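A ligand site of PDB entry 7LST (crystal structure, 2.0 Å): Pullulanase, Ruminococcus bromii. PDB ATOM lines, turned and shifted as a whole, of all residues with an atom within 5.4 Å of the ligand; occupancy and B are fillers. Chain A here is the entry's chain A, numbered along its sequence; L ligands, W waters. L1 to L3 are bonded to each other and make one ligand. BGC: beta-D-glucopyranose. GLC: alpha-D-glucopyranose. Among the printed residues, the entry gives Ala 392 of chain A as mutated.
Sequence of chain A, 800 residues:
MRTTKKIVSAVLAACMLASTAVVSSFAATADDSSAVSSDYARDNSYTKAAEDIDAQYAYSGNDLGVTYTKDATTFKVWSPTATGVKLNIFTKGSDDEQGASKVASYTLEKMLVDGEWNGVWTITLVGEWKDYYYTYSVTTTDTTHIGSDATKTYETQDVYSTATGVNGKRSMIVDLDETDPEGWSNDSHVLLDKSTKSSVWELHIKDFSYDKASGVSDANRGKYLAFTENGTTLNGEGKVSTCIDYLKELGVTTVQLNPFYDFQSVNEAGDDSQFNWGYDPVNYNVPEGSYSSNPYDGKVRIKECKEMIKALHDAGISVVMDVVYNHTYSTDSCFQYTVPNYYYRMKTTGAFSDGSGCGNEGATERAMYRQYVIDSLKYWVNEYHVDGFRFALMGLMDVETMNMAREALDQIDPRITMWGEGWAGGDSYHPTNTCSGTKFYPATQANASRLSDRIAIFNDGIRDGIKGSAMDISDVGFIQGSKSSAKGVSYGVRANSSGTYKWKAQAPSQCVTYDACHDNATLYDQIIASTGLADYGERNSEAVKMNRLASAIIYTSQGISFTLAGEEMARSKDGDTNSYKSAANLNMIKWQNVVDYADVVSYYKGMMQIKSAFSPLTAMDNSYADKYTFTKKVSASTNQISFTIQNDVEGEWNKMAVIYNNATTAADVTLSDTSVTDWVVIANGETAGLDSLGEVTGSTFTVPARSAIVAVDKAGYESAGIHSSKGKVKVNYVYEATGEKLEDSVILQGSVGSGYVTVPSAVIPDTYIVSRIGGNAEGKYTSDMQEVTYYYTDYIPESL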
ATOM      1  N   ASN A 276     -18.333 -29.114 -14.119  1.00  0.00           N
ATOM      2  CA  ASN A 276     -19.071 -28.010 -13.512  1.00  0.00           C
ATOM      3  C   ASN A 276     -19.481 -27.043 -14.621  1.00  0.00           C
ATOM      4  O   ASN A 276     -18.741 -26.865 -15.586  1.00  0.00           O
ATOM      5  CB  ASN A 276     -18.277 -27.323 -12.393  1.00  0.00           C
ATOM      6  CG  ASN A 276     -19.156 -26.581 -11.407  1.00  0.00           C
ATOM      7  OD1 ASN A 276     -19.710 -25.533 -11.715  1.00  0.00           O
ATOM      8  ND2 ASN A 276     -19.287 -27.125 -10.200  1.00  0.00           N
ATOM      9  N   TRP A 277     -20.667 -26.431 -14.479  1.00  0.00           N
ATOM     10  CA  TRP A 277     -21.115 -25.370 -15.364  1.00  0.00           C
ATOM     11  C   TRP A 277     -20.130 -24.207 -15.308  1.00  0.00           C
ATOM     12  O   TRP A 277     -19.825 -23.597 -16.334  1.00  0.00           O
ATOM     13  CB  TRP A 277     -22.534 -24.871 -15.007  1.00  0.00           C
ATOM     14  CG  TRP A 277     -23.659 -25.788 -15.386  1.00  0.00           C
ATOM     15  CD1 TRP A 277     -23.651 -26.787 -16.327  1.00  0.00           C
ATOM     16  CD2 TRP A 277     -24.991 -25.763 -14.846  1.00  0.00           C
ATOM     17  NE1 TRP A 277     -24.880 -27.394 -16.380  1.00  0.00           N
ATOM     18  CE2 TRP A 277     -25.718 -26.785 -15.487  1.00  0.00           C
ATOM     19  CE3 TRP A 277     -25.636 -24.987 -13.885  1.00  0.00           C
ATOM     20  CZ2 TRP A 277     -27.055 -27.053 -15.180  1.00  0.00           C
ATOM     21  CZ3 TRP A 277     -26.954 -25.243 -13.574  1.00  0.00           C
ATOM     22  CH2 TRP A 277     -27.652 -26.267 -14.223  1.00  0.00           C
ATOM     23  N   TYR A 279     -20.135 -21.447 -12.757  1.00  0.00           N
ATOM     24  CA  TYR A 279     -20.679 -20.156 -12.308  1.00  0.00           C
ATOM     25  C   TYR A 279     -19.980 -19.749 -10.998  1.00  0.00           C
ATOM     26  O   TYR A 279     -20.603 -19.216 -10.077  1.00  0.00           O
ATOM     27  CB  TYR A 279     -22.207 -20.227 -12.194  1.00  0.00           C
ATOM     28  CG  TYR A 279     -22.887 -20.341 -13.534  1.00  0.00           C
ATOM     29  CD1 TYR A 279     -22.969 -19.257 -14.384  1.00  0.00           C
ATOM     30  CD2 TYR A 279     -23.403 -21.549 -13.977  1.00  0.00           C
ATOM     31  CE1 TYR A 279     -23.555 -19.355 -15.628  1.00  0.00           C
ATOM     32  CE2 TYR A 279     -23.997 -21.670 -15.219  1.00  0.00           C
ATOM     33  CZ  TYR A 279     -24.084 -20.557 -16.053  1.00  0.00           C
ATOM     34  OH  TYR A 279     -24.657 -20.665 -17.273  1.00  0.00           O
ATOM     35  N   ASP A 280     -18.651 -19.926 -10.978  1.00  0.00           N
ATOM     36  CA  ASP A 280     -17.803 -19.839  -9.788  1.00  0.00           C
ATOM     37  C   ASP A 280     -16.538 -19.053 -10.143  1.00  0.00           C
ATOM     38  O   ASP A 280     -15.443 -19.599 -10.142  1.00  0.00           O
ATOM     39  CB  ASP A 280     -17.466 -21.229  -9.259  1.00  0.00           C
ATOM     40  CG  ASP A 280     -18.672 -22.138  -9.012  1.00  0.00           C
ATOM     41  OD1 ASP A 280     -19.623 -21.677  -8.328  1.00  0.00           O
ATOM     42  OD2 ASP A 280     -18.645 -23.295  -9.487  1.00  0.00           O
ATOM     43  N   ASP A 322     -21.331 -16.292 -21.851  1.00  0.00           N
ATOM     44  CA  ASP A 322     -21.944 -16.254 -20.531  1.00  0.00           C
ATOM     45  C   ASP A 322     -20.929 -15.620 -19.559  1.00  0.00           C
ATOM     46  O   ASP A 322     -19.792 -16.074 -19.486  1.00  0.00           O
ATOM     47  CB  ASP A 322     -22.344 -17.670 -20.113  1.00  0.00           C
ATOM     48  CG  ASP A 322     -23.352 -17.761 -18.976  1.00  0.00           C
ATOM     49  OD1 ASP A 322     -23.397 -16.832 -18.144  1.00  0.00           O
ATOM     50  OD2 ASP A 322     -24.076 -18.776 -18.933  1.00  0.00           O
ATOM     51  N   ASN A 326     -21.790 -10.664 -11.374  1.00  0.00           N
ATOM     52  CA  ASN A 326     -22.706 -10.475 -10.243  1.00  0.00           C
ATOM     53  C   ASN A 326     -22.132 -11.044  -8.931  1.00  0.00           C
ATOM     54  O   ASN A 326     -22.527 -10.593  -7.860  1.00  0.00           O
ATOM     55  CB  ASN A 326     -24.084 -11.060 -10.552  1.00  0.00           C
ATOM     56  CG  ASN A 326     -24.100 -12.569 -10.557  1.00  0.00           C
ATOM     57  OD1 ASN A 326     -24.046 -13.202  -9.505  1.00  0.00           O
ATOM     58  ND2 ASN A 326     -24.177 -13.169 -11.735  1.00  0.00           N
ATOM     59  N   HIS A 327     -21.244 -12.050  -9.016  1.00  0.00           N
ATOM     60  CA  HIS A 327     -20.593 -12.636  -7.826  1.00  0.00           C
ATOM     61  C   HIS A 327     -19.307 -13.374  -8.223  1.00  0.00           C
ATOM     62  O   HIS A 327     -19.161 -13.802  -9.363  1.00  0.00           O
ATOM     63  CB  HIS A 327     -21.559 -13.581  -7.090  1.00  0.00           C
ATOM     64  CG  HIS A 327     -21.636 -14.947  -7.685  1.00  0.00           C
ATOM     65  ND1 HIS A 327     -22.364 -15.223  -8.820  1.00  0.00           N
ATOM     66  CD2 HIS A 327     -21.049 -16.109  -7.326  1.00  0.00           C
ATOM     67  CE1 HIS A 327     -22.231 -16.495  -9.129  1.00  0.00           C
ATOM     68  NE2 HIS A 327     -21.433 -17.061  -8.229  1.00  0.00           N
ATOM     69  N   TYR A 329     -16.633 -16.686  -6.791  1.00  0.00           N
ATOM     70  CA  TYR A 329     -16.778 -17.962  -6.081  1.00  0.00           C
ATOM     71  C   TYR A 329     -16.775 -17.740  -4.552  1.00  0.00           C
ATOM     72  O   TYR A 329     -17.579 -18.340  -3.848  1.00  0.00           O
ATOM     73  CB  TYR A 329     -15.662 -18.952  -6.434  1.00  0.00           C
ATOM     74  CG  TYR A 329     -15.664 -20.184  -5.563  1.00  0.00           C
ATOM     75  CD1 TYR A 329     -16.723 -21.072  -5.606  1.00  0.00           C
ATOM     76  CD2 TYR A 329     -14.639 -20.441  -4.669  1.00  0.00           C
ATOM     77  CE1 TYR A 329     -16.757 -22.205  -4.803  1.00  0.00           C
ATOM     78  CE2 TYR A 329     -14.656 -21.569  -3.855  1.00  0.00           C
ATOM     79  CZ  TYR A 329     -15.714 -22.451  -3.922  1.00  0.00           C
ATOM     80  OH  TYR A 329     -15.745 -23.570  -3.148  1.00  0.00           O
ATOM     81  N   SER A 356     -26.933 -13.120  -4.681  1.00  0.00           N
ATOM     82  CA  SER A 356     -26.644 -14.162  -5.676  1.00  0.00           C
ATOM     83  C   SER A 356     -27.035 -15.542  -5.150  1.00  0.00           C
ATOM     84  O   SER A 356     -27.214 -16.481  -5.924  1.00  0.00           O
ATOM     85  CB  SER A 356     -25.183 -14.138  -6.054  1.00  0.00           C
ATOM     86  OG  SER A 356     -24.378 -14.513  -4.945  1.00  0.00           O
ATOM     87  N   GLY A 357     -27.126 -15.667  -3.819  1.00  0.00           N
ATOM     88  CA  GLY A 357     -27.288 -16.963  -3.153  1.00  0.00           C
ATOM     89  C   GLY A 357     -26.040 -17.821  -3.262  1.00  0.00           C
ATOM     90  O   GLY A 357     -26.110 -19.036  -3.037  1.00  0.00           O
ATOM     91  N   CYS A 358     -24.906 -17.207  -3.609  1.00  0.00           N
ATOM     92  CA  CYS A 358     -23.621 -17.884  -3.731  1.00  0.00           C
ATOM     93  C   CYS A 358     -22.609 -17.335  -2.702  1.00  0.00           C
ATOM     94  O   CYS A 358     -21.505 -17.875  -2.598  1.00  0.00           O
ATOM     95  CB  CYS A 358     -23.066 -17.764  -5.137  1.00  0.00           C
ATOM     96  SG  CYS A 358     -24.064 -18.645  -6.374  1.00  0.00           S
ATOM     97  N   GLY A 359     -22.988 -16.300  -1.950  1.00  0.00           N
ATOM     98  CA  GLY A 359     -22.193 -15.793  -0.821  1.00  0.00           C
ATOM     99  C   GLY A 359     -21.902 -14.299  -0.870  1.00  0.00           C
ATOM    100  O   GLY A 359     -21.577 -13.709   0.156  1.00  0.00           O
ATOM    101  N   ARG A 390     -24.200 -12.902 -22.454  1.00  0.00           N
ATOM    102  CA  ARG A 390     -25.335 -13.286 -21.622  1.00  0.00           C
ATOM    103  C   ARG A 390     -24.957 -13.022 -20.157  1.00  0.00           C
ATOM    104  O   ARG A 390     -24.051 -13.645 -19.634  1.00  0.00           O
ATOM    105  CB  ARG A 390     -25.688 -14.762 -21.853  1.00  0.00           C
ATOM    106  CG  ARG A 390     -26.783 -15.308 -20.945  1.00  0.00           C
ATOM    107  CD  ARG A 390     -26.265 -16.037 -19.713  1.00  0.00           C
ATOM    108  NE  ARG A 390     -27.297 -16.803 -19.040  1.00  0.00           N
ATOM    109  CZ  ARG A 390     -27.212 -17.262 -17.791  1.00  0.00           C
ATOM    110  NH1 ARG A 390     -26.123 -17.042 -17.074  1.00  0.00           N
ATOM    111  NH2 ARG A 390     -28.230 -17.938 -17.276  1.00  0.00           N
ATOM    112  N   ALA A 392     -25.346 -13.277 -16.361  1.00  0.00           N
ATOM    113  CA  ALA A 392     -25.871 -14.053 -15.239  1.00  0.00           C
ATOM    114  C   ALA A 392     -26.425 -13.080 -14.192  1.00  0.00           C
ATOM    115  O   ALA A 392     -25.777 -12.088 -13.863  1.00  0.00           O
ATOM    116  CB  ALA A 392     -24.787 -14.918 -14.657  1.00  0.00           C
ATOM    117  N   LEU A 393     -27.627 -13.383 -13.678  1.00  0.00           N
ATOM    118  CA  LEU A 393     -28.326 -12.574 -12.680  1.00  0.00           C
ATOM    119  C   LEU A 393     -28.086 -11.085 -12.939  1.00  0.00           C
ATOM    120  O   LEU A 393     -27.469 -10.383 -12.127  1.00  0.00           O
ATOM    121  CB  LEU A 393     -27.842 -12.977 -11.284  1.00  0.00           C
ATOM    122  CG  LEU A 393     -28.090 -14.425 -10.870  1.00  0.00           C
ATOM    123  CD1 LEU A 393     -27.617 -14.663  -9.442  1.00  0.00           C
ATOM    124  CD2 LEU A 393     -29.563 -14.805 -11.004  1.00  0.00           C
ATOM    125  N   GLU A 421     -30.520 -12.471 -17.392  1.00  0.00           N
ATOM    126  CA  GLU A 421     -31.607 -12.812 -16.478  1.00  0.00           C
ATOM    127  C   GLU A 421     -32.056 -11.554 -15.739  1.00  0.00           C
ATOM    128  O   GLU A 421     -31.292 -10.989 -14.976  1.00  0.00           O
ATOM    129  CB  GLU A 421     -31.130 -13.818 -15.424  1.00  0.00           C
ATOM    130  CG  GLU A 421     -30.824 -15.207 -15.954  1.00  0.00           C
ATOM    131  CD  GLU A 421     -30.121 -16.085 -14.930  1.00  0.00           C
ATOM    132  OE1 GLU A 421     -30.623 -17.195 -14.644  1.00  0.00           O
ATOM    133  OE2 GLU A 421     -29.084 -15.645 -14.413  1.00  0.00           O
ATOM    134  N   HIS A 518     -30.062 -24.339 -19.718  1.00  0.00           N
ATOM    135  CA  HIS A 518     -29.222 -25.256 -18.946  1.00  0.00           C
ATOM    136  C   HIS A 518     -29.819 -25.457 -17.539  1.00  0.00           C
ATOM    137  O   HIS A 518     -29.691 -26.536 -16.965  1.00  0.00           O
ATOM    138  CB  HIS A 518     -27.771 -24.746 -18.888  1.00  0.00           C
ATOM    139  CG  HIS A 518     -27.584 -23.548 -18.013  1.00  0.00           C
ATOM    140  ND1 HIS A 518     -27.782 -22.270 -18.471  1.00  0.00           N
ATOM    141  CD2 HIS A 518     -27.247 -23.451 -16.710  1.00  0.00           C
ATOM    142  CE1 HIS A 518     -27.553 -21.420 -17.487  1.00  0.00           C
ATOM    143  NE2 HIS A 518     -27.234 -22.118 -16.393  1.00  0.00           N
ATOM    144  N   ASP A 519     -30.445 -24.412 -16.994  1.00  0.00           N
ATOM    145  CA  ASP A 519     -31.025 -24.460 -15.654  1.00  0.00           C
ATOM    146  C   ASP A 519     -32.287 -25.334 -15.683  1.00  0.00           C
ATOM    147  O   ASP A 519     -32.935 -25.472 -16.711  1.00  0.00           O
ATOM    148  CB  ASP A 519     -31.358 -23.062 -15.123  1.00  0.00           C
ATOM    149  CG  ASP A 519     -30.190 -22.357 -14.475  1.00  0.00           C
ATOM    150  OD1 ASP A 519     -29.519 -23.003 -13.630  1.00  0.00           O
ATOM    151  OD2 ASP A 519     -29.937 -21.180 -14.810  1.00  0.00           O
ATOM    152  N   ASN A 578     -30.924 -29.732 -11.800  1.00  0.00           N
ATOM    153  CA  ASN A 578     -29.837 -28.811 -11.460  1.00  0.00           C
ATOM    154  C   ASN A 578     -28.494 -29.527 -11.624  1.00  0.00           C
ATOM    155  O   ASN A 578     -27.848 -29.891 -10.632  1.00  0.00           O
ATOM    156  CB  ASN A 578     -29.992 -28.229 -10.049  1.00  0.00           C
ATOM    157  CG  ASN A 578     -29.044 -27.080  -9.786  1.00  0.00           C
ATOM    158  OD1 ASN A 578     -28.661 -26.362 -10.708  1.00  0.00           O
ATOM    159  ND2 ASN A 578     -28.664 -26.890  -8.532  1.00  0.00           N
ATOM    160  N   TYR A 580     -25.470 -28.915 -12.398  1.00  0.00           N
ATOM    161  CA  TYR A 580     -24.275 -28.057 -12.409  1.00  0.00           C
ATOM    162  C   TYR A 580     -22.998 -28.840 -12.061  1.00  0.00           C
ATOM    163  O   TYR A 580     -21.946 -28.550 -12.638  1.00  0.00           O
ATOM    164  CB  TYR A 580     -24.463 -26.824 -11.520  1.00  0.00           C
ATOM    165  CG  TYR A 580     -24.366 -27.039 -10.031  1.00  0.00           C
ATOM    166  CD1 TYR A 580     -25.427 -27.563  -9.306  1.00  0.00           C
ATOM    167  CD2 TYR A 580     -23.244 -26.645  -9.320  1.00  0.00           C
ATOM    168  CE1 TYR A 580     -25.365 -27.726  -7.938  1.00  0.00           C
ATOM    169  CE2 TYR A 580     -23.150 -26.801  -7.950  1.00  0.00           C
ATOM    170  CZ  TYR A 580     -24.221 -27.350  -7.258  1.00  0.00           C
ATOM    171  OH  TYR A 580     -24.152 -27.512  -5.902  1.00  0.00           O
HETATM  172  C2  BGC L   1     -27.045 -19.528 -13.899  1.00  0.00           C
HETATM  173  C3  BGC L   1     -27.262 -20.626 -12.863  1.00  0.00           C
HETATM  174  C4  BGC L   1     -26.298 -20.407 -11.702  1.00  0.00           C
HETATM  175  C5  BGC L   1     -26.513 -18.997 -11.134  1.00  0.00           C
HETATM  176  C6  BGC L   1     -25.532 -18.653 -10.009  1.00  0.00           C
HETATM  177  C1  BGC L   1     -27.248 -18.163 -13.254  1.00  0.00           C
HETATM  178  O1  BGC L   1     -26.977 -17.145 -14.208  1.00  0.00           O
HETATM  179  O2  BGC L   1     -27.955 -19.661 -15.006  1.00  0.00           O
HETATM  180  O3  BGC L   1     -27.091 -21.917 -13.463  1.00  0.00           O
HETATM  181  O4  BGC L   1     -26.517 -21.353 -10.662  1.00  0.00           O
HETATM  182  O5  BGC L   1     -26.362 -18.014 -12.152  1.00  0.00           O
HETATM  183  O6  BGC L   1     -25.920 -17.415  -9.384  1.00  0.00           O
HETATM  184  C1  GLC L   2     -25.685 -22.525 -10.786  1.00  0.00           C
HETATM  185  C2  GLC L   2     -26.399 -23.655 -10.041  1.00  0.00           C
HETATM  186  C3  GLC L   2     -26.353 -23.388  -8.541  1.00  0.00           C
HETATM  187  C4  GLC L   2     -24.917 -23.204  -8.051  1.00  0.00           C
HETATM  188  C5  GLC L   2     -24.258 -22.089  -8.877  1.00  0.00           C
HETATM  189  C6  GLC L   2     -22.788 -21.852  -8.503  1.00  0.00           C
HETATM  190  O2  GLC L   2     -27.760 -23.778 -10.483  1.00  0.00           O
HETATM  191  O3  GLC L   2     -26.978 -24.464  -7.846  1.00  0.00           O
HETATM  192  O4  GLC L   2     -24.959 -22.845  -6.659  1.00  0.00           O
HETATM  193  O5  GLC L   2     -24.347 -22.369 -10.281  1.00  0.00           O
HETATM  194  O6  GLC L   2     -21.947 -22.919  -8.940  1.00  0.00           O
HETATM  195  C1  GLC L   3     -24.388 -23.852  -5.780  1.00  0.00           C
HETATM  196  C2  GLC L   3     -25.038 -23.754  -4.403  1.00  0.00           C
HETATM  197  C3  GLC L   3     -24.666 -22.431  -3.747  1.00  0.00           C
HETATM  198  C4  GLC L   3     -23.160 -22.417  -3.542  1.00  0.00           C
HETATM  199  C5  GLC L   3     -22.481 -22.587  -4.900  1.00  0.00           C
HETATM  200  C6  GLC L   3     -20.950 -22.643  -4.769  1.00  0.00           C
HETATM  201  O2  GLC L   3     -26.456 -23.854  -4.522  1.00  0.00           O
HETATM  202  O3  GLC L   3     -25.343 -22.280  -2.504  1.00  0.00           O
HETATM  203  O4  GLC L   3     -22.758 -21.171  -2.965  1.00  0.00           O
HETATM  204  O5  GLC L   3     -22.969 -23.756  -5.603  1.00  0.00           O
HETATM  205  O6  GLC L   3     -20.536 -23.660  -3.843  1.00  0.00           O
HETATM  206  O   HOH W   1     -21.754 -26.381  -4.675  1.00  0.00           O
HETATM  207  O   HOH W   2     -20.160 -25.228  -8.416  1.00  0.00           O
HETATM  208  O   HOH W   3     -27.732 -18.295  -7.904  1.00  0.00           O
HETATM  209  O   HOH W   4     -29.520 -21.891  -9.953  1.00  0.00           O
HETATM  210  O   HOH W   5     -24.651 -16.019 -11.316  1.00  0.00           O
HETATM  211  O   HOH W   6     -26.671 -27.201  -4.315  1.00  0.00           O
HETATM  212  O   HOH W   7     -21.769 -23.609 -11.536  1.00  0.00           O
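NE2 of His 518 sits at hydrogen-bond distance from OD2 of Asp 519 (3.3 Å). The side-chain carboxylate of Glu 421 sits at hydrogen-bond distance from the backbone NH of Leu 393 (2.8 Å). The side-chain carboxylate of Asp 280 sits close to the side-chain amide oxygen of Asn 276 (3.3 Å). The guanidinium group of Arg 390 is in salt-bridge range of the side-chain carboxylate of Asp 322 (2.9 Å). A ring nitrogen (NE2) of His 518 sits close to the side-chain hydroxyl (OH) of Tyr 279 (3.1 Å). ND2 of Asn 326 sits at hydrogen-bond distance from O of Ala 392 (2.9 Å). SG of Cys 358 sits close to NE2 of His 327, 3.6 Å away. The side-chain carboxylate of Asp 322 is in hydrogen-bond range of the side-chain hydroxyl of Tyr 279, at 2.6 Å.
Residues that only touch the ligand: Ala 392 (3.2 Å), Leu 393 (3.2 Å), Trp 277 (3.3 Å), Tyr 279 (3.6 Å), Tyr 580 (3.6 Å), Ser 356 (3.8 Å) and His 327 (3.8 Å). 15 residues have an atom within 4 Å of the ligand: Trp 277, Tyr 279, Asp 280, His 327, Ser 356, Gly 357, Cys 358, Arg 390, Ala 392, Leu 393, Glu 421, His 518, Asp 519, Asn 578 and Tyr 580. The nearest printed residue that does not touch the ligand is Tyr 329 (4.2 Å).
The side-chain carboxylate of Asp 519 is in hydrogen-bond range of an oxygen (O2) of BGC L1. The side-chain carboxylate (OE2) of Glu 421 is in hydrogen-bond range of an oxygen (O1) of BGC L1, at 2.6 Å. The side-chain carboxylate of Asp 280 is in hydrogen-bond range of an oxygen (O6) of GLC L2, at 2.7 Å. The side-chain amide oxygen of Asn 578 lies within hydrogen-bond range of an oxygen (O2) of GLC L2 (2.7 Å). An oxygen (O2) of BGC L1 lies within hydrogen-bond range of the guanidinium group (NH2) of Arg 390 (2.9 Å). A ring nitrogen (NE2) of His 518 lies within hydrogen-bond range of an oxygen (O2) of BGC L1, 2.9 Å away. O3 of GLC L3 is in hydrogen-bond range of O of Gly 357, 3.4 Å away. An oxygen (O6) of BGC L1 is in hydrogen-bond range of the side-chain sulfur (SG) of Cys 358.
Water W3 bridges an oxygen (O6) of BGC L1 (2.5 Å) and the backbone carbonyl oxygen (O) of Ser 356 (2.7 Å). Water W7 lies within hydrogen-bond range of an oxygen (O6) of GLC L2 (2.7 Å), the side-chain amide oxygen (OD1) of Asn 276 (2.8 Å) and the backbone NH (N) of Tyr 279 (3.0 Å). Water W5 lies within hydrogen-bond range of an oxygen (O6) of BGC L1 (2.7 Å), the side-chain amide nitrogen of Asn 326 (2.9 Å) and a ring nitrogen (ND1) of His 327 (3.5 Å). Water W2 lies within hydrogen-bond range of the side-chain carboxylate (OD2) of Asp 280, the side-chain amide nitrogen (ND2) of Asn 276 and an oxygen (O6) of GLC L2. Water W1 bridges OH of Tyr 580 (2.9 Å) and O5 of GLC L3 (3.0 Å). Water W6 bridges OH of Tyr 580 (3.0 Å) and O2 of GLC L3 (3.4 Å).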
